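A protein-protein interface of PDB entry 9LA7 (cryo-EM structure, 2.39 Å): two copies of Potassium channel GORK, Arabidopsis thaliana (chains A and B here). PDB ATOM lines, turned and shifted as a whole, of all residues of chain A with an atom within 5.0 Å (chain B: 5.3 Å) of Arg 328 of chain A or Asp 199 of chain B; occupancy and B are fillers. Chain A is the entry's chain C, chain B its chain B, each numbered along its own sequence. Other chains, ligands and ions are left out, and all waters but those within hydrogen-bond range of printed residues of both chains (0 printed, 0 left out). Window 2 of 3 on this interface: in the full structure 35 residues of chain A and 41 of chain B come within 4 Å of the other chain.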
ATOM      1  N   ASN A 323     -37.389 -17.389 -25.546  1.00  0.00           N
ATOM      2  CA  ASN A 323     -36.456 -16.376 -24.980  1.00  0.00           C
ATOM      3  C   ASN A 323     -35.027 -16.840 -25.263  1.00  0.00           C
ATOM      4  O   ASN A 323     -34.172 -15.975 -25.539  1.00  0.00           O
ATOM      5  CB  ASN A 323     -36.724 -16.135 -23.500  1.00  0.00           C
ATOM      6  CG  ASN A 323     -38.084 -15.518 -23.276  1.00  0.00           C
ATOM      7  OD1 ASN A 323     -39.104 -16.112 -23.645  1.00  0.00           O
ATOM      8  ND2 ASN A 323     -38.123 -14.332 -22.688  1.00  0.00           N
ATOM      9  N   THR A 324     -34.785 -18.152 -25.216  1.00  0.00           N
ATOM     10  CA  THR A 324     -33.452 -18.696 -25.543  1.00  0.00           C
ATOM     11  C   THR A 324     -33.061 -18.230 -26.926  1.00  0.00           C
ATOM     12  O   THR A 324     -31.894 -17.835 -27.107  1.00  0.00           O
ATOM     13  CB  THR A 324     -33.516 -20.218 -25.467  1.00  0.00           C
ATOM     14  OG1 THR A 324     -33.831 -20.507 -24.108  1.00  0.00           O
ATOM     15  CG2 THR A 324     -32.204 -20.879 -25.850  1.00  0.00           C
ATOM     16  N   GLU A 325     -33.997 -18.279 -27.877  1.00  0.00           N
ATOM     17  CA  GLU A 325     -33.724 -17.823 -29.266  1.00  0.00           C
ATOM     18  C   GLU A 325     -33.552 -16.296 -29.278  1.00  0.00           C
ATOM     19  O   GLU A 325     -32.576 -15.815 -29.891  1.00  0.00           O
ATOM     20  CB  GLU A 325     -34.865 -18.270 -30.179  1.00  0.00           C
ATOM     21  CG  GLU A 325     -34.746 -17.762 -31.611  1.00  0.00           C
ATOM     22  CD  GLU A 325     -35.852 -18.302 -32.498  1.00  0.00           C
ATOM     23  OE1 GLU A 325     -36.665 -19.105 -31.996  1.00  0.00           O
ATOM     24  OE2 GLU A 325     -35.909 -17.915 -33.683  1.00  0.00           O
ATOM     25  N   ARG A 326     -34.464 -15.567 -28.630  1.00  0.00           N
ATOM     26  CA  ARG A 326     -34.320 -14.091 -28.537  1.00  0.00           C
ATOM     27  C   ARG A 326     -32.920 -13.782 -27.988  1.00  0.00           C
ATOM     28  O   ARG A 326     -32.303 -12.803 -28.457  1.00  0.00           O
ATOM     29  CB  ARG A 326     -35.416 -13.496 -27.648  1.00  0.00           C
ATOM     30  CG  ARG A 326     -36.630 -12.981 -28.407  1.00  0.00           C
ATOM     31  CD  ARG A 326     -37.511 -14.099 -28.936  1.00  0.00           C
ATOM     32  NE  ARG A 326     -38.137 -14.853 -27.846  1.00  0.00           N
ATOM     33  CZ  ARG A 326     -39.445 -14.944 -27.655  1.00  0.00           C
ATOM     34  NH1 ARG A 326     -40.274 -14.277 -28.436  1.00  0.00           N
ATOM     35  NH2 ARG A 326     -39.922 -15.700 -26.683  1.00  0.00           N
ATOM     36  N   PHE A 327     -32.440 -14.595 -27.048  1.00  0.00           N
ATOM     37  CA  PHE A 327     -31.114 -14.414 -26.474  1.00  0.00           C
ATOM     38  C   PHE A 327     -30.027 -14.781 -27.473  1.00  0.00           C
ATOM     39  O   PHE A 327     -28.992 -14.117 -27.543  1.00  0.00           O
ATOM     40  CB  PHE A 327     -30.963 -15.243 -25.199  1.00  0.00           C
ATOM     41  CG  PHE A 327     -29.535 -15.480 -24.811  1.00  0.00           C
ATOM     42  CD1 PHE A 327     -28.801 -14.483 -24.192  1.00  0.00           C
ATOM     43  CD2 PHE A 327     -28.919 -16.689 -25.089  1.00  0.00           C
ATOM     44  CE1 PHE A 327     -27.485 -14.693 -23.846  1.00  0.00           C
ATOM     45  CE2 PHE A 327     -27.601 -16.902 -24.746  1.00  0.00           C
ATOM     46  CZ  PHE A 327     -26.885 -15.902 -24.125  1.00  0.00           C
ATOM     47  N   ARG A 328     -30.230 -15.853 -28.237  1.00  0.00           N
ATOM     48  CA  ARG A 328     -29.252 -16.266 -29.235  1.00  0.00           C
ATOM     49  C   ARG A 328     -29.089 -15.206 -30.320  1.00  0.00           C
ATOM     50  O   ARG A 328     -27.967 -14.902 -30.741  1.00  0.00           O
ATOM     51  CB  ARG A 328     -29.654 -17.604 -29.857  1.00  0.00           C
ATOM     52  CG  ARG A 328     -29.397 -18.806 -28.964  1.00  0.00           C
ATOM     53  CD  ARG A 328     -27.935 -19.214 -28.988  1.00  0.00           C
ATOM     54  NE  ARG A 328     -27.550 -19.805 -30.264  1.00  0.00           N
ATOM     55  CZ  ARG A 328     -26.739 -19.229 -31.141  1.00  0.00           C
ATOM     56  NH1 ARG A 328     -26.206 -18.040 -30.912  1.00  0.00           N
ATOM     57  NH2 ARG A 328     -26.454 -19.862 -32.275  1.00  0.00           N
ATOM     58  N   ASP A 329     -30.205 -14.639 -30.781  1.00  0.00           N
ATOM     59  CA  ASP A 329     -30.128 -13.585 -31.790  1.00  0.00           C
ATOM     60  C   ASP A 329     -29.437 -12.338 -31.247  1.00  0.00           C
ATOM     61  O   ASP A 329     -28.621 -11.719 -31.945  1.00  0.00           O
ATOM     62  CB  ASP A 329     -31.527 -13.238 -32.300  1.00  0.00           C
ATOM     63  CG  ASP A 329     -31.599 -13.206 -33.813  1.00  0.00           C
ATOM     64  OD1 ASP A 329     -30.605 -13.596 -34.462  1.00  0.00           O
ATOM     65  OD2 ASP A 329     -32.644 -12.787 -34.354  1.00  0.00           O
ATOM     66  N   LYS A 330     -29.748 -11.960 -30.006  1.00  0.00           N
ATOM     67  CA  LYS A 330     -29.072 -10.822 -29.389  1.00  0.00           C
ATOM     68  C   LYS A 330     -27.584 -11.103 -29.215  1.00  0.00           C
ATOM     69  O   LYS A 330     -26.745 -10.218 -29.415  1.00  0.00           O
ATOM     70  CB  LYS A 330     -29.746 -10.485 -28.058  1.00  0.00           C
ATOM     71  CG  LYS A 330     -28.818 -10.148 -26.911  1.00  0.00           C
ATOM     72  CD  LYS A 330     -29.552  -9.298 -25.883  1.00  0.00           C
ATOM     73  CE  LYS A 330     -29.657 -10.005 -24.543  1.00  0.00           C
ATOM     74  NZ  LYS A 330     -30.013  -9.069 -23.442  1.00  0.00           N
ATOM     75  N   MET A 331     -27.240 -12.341 -28.853  1.00  0.00           N
ATOM     76  CA  MET A 331     -25.848 -12.772 -28.792  1.00  0.00           C
ATOM     77  C   MET A 331     -25.150 -12.572 -30.126  1.00  0.00           C
ATOM     78  O   MET A 331     -24.041 -12.036 -30.187  1.00  0.00           O
ATOM     79  CB  MET A 331     -25.782 -14.246 -28.378  1.00  0.00           C
ATOM     80  CG  MET A 331     -24.404 -14.741 -27.956  1.00  0.00           C
ATOM     81  SD  MET A 331     -23.282 -13.469 -27.358  1.00  0.00           S
ATOM     82  CE  MET A 331     -23.984 -13.176 -25.745  1.00  0.00           C
ATOM     83  N   ASN A 332     -25.785 -13.017 -31.209  1.00  0.00           N
ATOM     84  CA  ASN A 332     -25.173 -12.882 -32.525  1.00  0.00           C
ATOM     85  C   ASN A 332     -24.988 -11.416 -32.898  1.00  0.00           C
ATOM     86  O   ASN A 332     -23.961 -11.039 -33.472  1.00  0.00           O
ATOM     87  CB  ASN A 332     -26.011 -13.614 -33.574  1.00  0.00           C
ATOM     88  CG  ASN A 332     -26.209 -15.078 -33.235  1.00  0.00           C
ATOM     89  OD1 ASN A 332     -25.463 -15.647 -32.437  1.00  0.00           O
ATOM     90  ND2 ASN A 332     -27.214 -15.698 -33.842  1.00  0.00           N
ATOM     91  N   ARG B 195     -24.938 -27.955 -25.724  1.00  0.00           N
ATOM     92  CA  ARG B 195     -23.690 -27.206 -25.816  1.00  0.00           C
ATOM     93  C   ARG B 195     -23.514 -26.596 -27.201  1.00  0.00           C
ATOM     94  O   ARG B 195     -23.005 -25.478 -27.335  1.00  0.00           O
ATOM     95  CB  ARG B 195     -22.503 -28.108 -25.475  1.00  0.00           C
ATOM     96  CG  ARG B 195     -22.553 -28.709 -24.083  1.00  0.00           C
ATOM     97  CD  ARG B 195     -21.227 -29.356 -23.714  1.00  0.00           C
ATOM     98  NE  ARG B 195     -21.388 -30.756 -23.338  1.00  0.00           N
ATOM     99  CZ  ARG B 195     -20.925 -31.779 -24.042  1.00  0.00           C
ATOM    100  NH1 ARG B 195     -20.255 -31.597 -25.168  1.00  0.00           N
ATOM    101  NH2 ARG B 195     -21.139 -33.017 -23.606  1.00  0.00           N
ATOM    102  N   LEU B 196     -23.926 -27.321 -28.242  1.00  0.00           N
ATOM    103  CA  LEU B 196     -23.805 -26.813 -29.603  1.00  0.00           C
ATOM    104  C   LEU B 196     -24.747 -25.639 -29.837  1.00  0.00           C
ATOM    105  O   LEU B 196     -24.449 -24.745 -30.638  1.00  0.00           O
ATOM    106  CB  LEU B 196     -24.086 -27.936 -30.600  1.00  0.00           C
ATOM    107  CG  LEU B 196     -23.855 -27.654 -32.082  1.00  0.00           C
ATOM    108  CD1 LEU B 196     -22.371 -27.571 -32.381  1.00  0.00           C
ATOM    109  CD2 LEU B 196     -24.516 -28.726 -32.930  1.00  0.00           C
ATOM    110  N   GLU B 197     -25.894 -25.630 -29.155  1.00  0.00           N
ATOM    111  CA  GLU B 197     -26.823 -24.512 -29.280  1.00  0.00           C
ATOM    112  C   GLU B 197     -26.201 -23.220 -28.768  1.00  0.00           C
ATOM    113  O   GLU B 197     -26.378 -22.155 -29.370  1.00  0.00           O
ATOM    114  CB  GLU B 197     -28.118 -24.814 -28.528  1.00  0.00           C
ATOM    115  CG  GLU B 197     -29.336 -24.919 -29.422  1.00  0.00           C
ATOM    116  CD  GLU B 197     -30.506 -25.596 -28.737  1.00  0.00           C
ATOM    117  OE1 GLU B 197     -30.595 -25.516 -27.493  1.00  0.00           O
ATOM    118  OE2 GLU B 197     -31.339 -26.201 -29.441  1.00  0.00           O
ATOM    119  N   LYS B 198     -25.468 -23.294 -27.658  1.00  0.00           N
ATOM    120  CA  LYS B 198     -24.795 -22.125 -27.110  1.00  0.00           C
ATOM    121  C   LYS B 198     -23.471 -21.889 -27.825  1.00  0.00           C
ATOM    122  O   LYS B 198     -22.424 -21.757 -27.183  1.00  0.00           O
ATOM    123  CB  LYS B 198     -24.567 -22.296 -25.607  1.00  0.00           C
ATOM    124  CG  LYS B 198     -25.673 -23.057 -24.899  1.00  0.00           C
ATOM    125  CD  LYS B 198     -25.866 -22.566 -23.475  1.00  0.00           C
ATOM    126  CE  LYS B 198     -26.181 -23.716 -22.535  1.00  0.00           C
ATOM    127  NZ  LYS B 198     -25.065 -24.700 -22.466  1.00  0.00           N
ATOM    128  N   ASP B 199     -23.510 -21.836 -29.155  1.00  0.00           N
ATOM    129  CA  ASP B 199     -22.328 -21.602 -29.971  1.00  0.00           C
ATOM    130  C   ASP B 199     -22.678 -20.597 -31.056  1.00  0.00           C
ATOM    131  O   ASP B 199     -23.693 -20.750 -31.742  1.00  0.00           O
ATOM    132  CB  ASP B 199     -21.815 -22.904 -30.597  1.00  0.00           C
ATOM    133  CG  ASP B 199     -20.604 -23.459 -29.876  1.00  0.00           C
ATOM    134  OD1 ASP B 199     -20.484 -23.241 -28.653  1.00  0.00           O
ATOM    135  OD2 ASP B 199     -19.770 -24.119 -30.534  1.00  0.00           O
ATOM    136  N   THR B 200     -21.839 -19.571 -31.206  1.00  0.00           N
ATOM    137  CA  THR B 200     -22.113 -18.518 -32.177  1.00  0.00           C
ATOM    138  C   THR B 200     -21.901 -18.976 -33.614  1.00  0.00           C
ATOM    139  O   THR B 200     -22.397 -18.322 -34.538  1.00  0.00           O
ATOM    140  CB  THR B 200     -21.234 -17.299 -31.890  1.00  0.00           C
ATOM    141  OG1 THR B 200     -19.981 -17.441 -32.568  1.00  0.00           O
ATOM    142  CG2 THR B 200     -20.982 -17.168 -30.396  1.00  0.00           C
ATOM    143  N   ARG B 201     -21.181 -20.079 -33.826  1.00  0.00           N
ATOM    144  CA  ARG B 201     -20.857 -20.503 -35.185  1.00  0.00           C
ATOM    145  C   ARG B 201     -22.081 -21.044 -35.915  1.00  0.00           C
ATOM    146  O   ARG B 201     -22.182 -20.922 -37.142  1.00  0.00           O
ATOM    147  CB  ARG B 201     -19.746 -21.554 -35.157  1.00  0.00           C
ATOM    148  CG  ARG B 201     -18.935 -21.579 -33.871  1.00  0.00           C
ATOM    149  CD  ARG B 201     -17.806 -22.598 -33.952  1.00  0.00           C
ATOM    150  NE  ARG B 201     -16.816 -22.245 -34.962  1.00  0.00           N
ATOM    151  CZ  ARG B 201     -15.799 -23.019 -35.319  1.00  0.00           C
ATOM    152  NH1 ARG B 201     -15.605 -24.205 -34.766  1.00  0.00           N
ATOM    153  NH2 ARG B 201     -14.955 -22.591 -36.255  1.00  0.00           N
ATOM    154  N   ILE B 202     -23.021 -21.641 -35.186  1.00  0.00           N
ATOM    155  CA  ILE B 202     -24.144 -22.355 -35.782  1.00  0.00           C
ATOM    156  C   ILE B 202     -25.448 -21.731 -35.300  1.00  0.00           C
ATOM    157  O   ILE B 202     -25.585 -21.389 -34.119  1.00  0.00           O
ATOM    158  CB  ILE B 202     -24.083 -23.861 -35.446  1.00  0.00           C
ATOM    159  CG1 ILE B 202     -23.030 -24.551 -36.314  1.00  0.00           C
ATOM    160  CG2 ILE B 202     -25.421 -24.527 -35.680  1.00  0.00           C
ATOM    161  CD1 ILE B 202     -22.891 -26.035 -36.044  1.00  0.00           C
ATOM    162  N   ASN B 203     -26.399 -21.578 -36.221  1.00  0.00           N
ATOM    163  CA  ASN B 203     -27.676 -20.942 -35.917  1.00  0.00           C
ATOM    164  C   ASN B 203     -28.458 -21.756 -34.889  1.00  0.00           C
ATOM    165  O   ASN B 203     -28.329 -22.979 -34.799  1.00  0.00           O
ATOM    166  CB  ASN B 203     -28.494 -20.782 -37.204  1.00  0.00           C
ATOM    167  CG  ASN B 203     -29.765 -19.965 -37.009  1.00  0.00           C
ATOM    168  OD1 ASN B 203     -30.492 -20.131 -36.029  1.00  0.00           O
ATOM    169  ND2 ASN B 203     -30.040 -19.078 -37.958  1.00  0.00           N
ATOM    170  N   TYR B 204     -29.279 -21.051 -34.106  1.00  0.00           N
ATOM    171  CA  TYR B 204     -30.099 -21.713 -33.094  1.00  0.00           C
ATOM    172  C   TYR B 204     -31.179 -22.575 -33.733  1.00  0.00           C
ATOM    173  O   TYR B 204     -31.359 -23.742 -33.364  1.00  0.00           O
ATOM    174  CB  TYR B 204     -30.737 -20.673 -32.175  1.00  0.00           C
ATOM    175  CG  TYR B 204     -31.696 -21.267 -31.168  1.00  0.00           C
ATOM    176  CD1 TYR B 204     -31.248 -22.122 -30.174  1.00  0.00           C
ATOM    177  CD2 TYR B 204     -33.056 -21.002 -31.237  1.00  0.00           C
ATOM    178  CE1 TYR B 204     -32.122 -22.673 -29.257  1.00  0.00           C
ATOM    179  CE2 TYR B 204     -33.938 -21.552 -30.327  1.00  0.00           C
ATOM    180  CZ  TYR B 204     -33.466 -22.386 -29.339  1.00  0.00           C
ATOM    181  OH  TYR B 204     -34.342 -22.934 -28.430  1.00  0.00           O
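Among the printed residues, merely in contact across the chains: Thr 324 of chain A with Tyr 204 of chain B (3.9 Å), Glu 325 of chain A with Tyr 204 of chain B (3.4 Å), Arg 328 of chain A with Asn 203 of chain B (3.8 Å) and Arg 328 of chain A with Tyr 204 of chain B (3.6 Å).
Printed residues of chain B that touch a printed residue of chain A: Glu 197, Asp 199, Ile 202, Asn 203 and Tyr 204. Among the printed residues, no Asp or Glu carboxylate lies within 4 Å of a Lys or Arg side-chain nitrogen of the other chain.
The guanidinium group of Arg 328 of chain A is in hydrogen-bond range of the side-chain amide oxygen of Asn 332 of chain A (2.9 Å).
Of chain A, only Arg 328 comes within 4 Å of Asp 199 of chain B. Of the printed residues of chain A, Glu 197 of chain B touches Arg 328 (2.8 Å). Of the printed residues of chain B, Glu 325 of chain A touches Tyr 204 (3.4 Å). Of the printed residues of chain A, Tyr 204 of chain B touches Thr 324 (3.9 Å), Glu 325 (3.4 Å) and Arg 328 (3.6 Å). Printed residues of chain A within 4 Å of Ile 202 of chain B: Arg 328. Of the printed residues of chain A, Asn 203 of chain B touches Arg 328. Arg 195 of chain B touches none of the printed residues of chain A. The nearest residue of chain B that does not touch Arg 328 of chain A is Thr 200 of chain B (4.3 Å).
No position is printed for both chains.
The guanidinium group (NE) of Arg 328 of chain A is in hydrogen-bond range of the backbone carbonyl oxygen (O) of Glu 197 of chain B, 2.8 Å away. O of Asp 199 of chain B is in hydrogen-bond range of NH2 of Arg 328 of chain A (2.9 Å). The backbone carbonyl oxygen (O) of Ile 202 of chain B is in hydrogen-bond range of the guanidinium group (NH2) of Arg 328 of chain A (2.5 Å).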
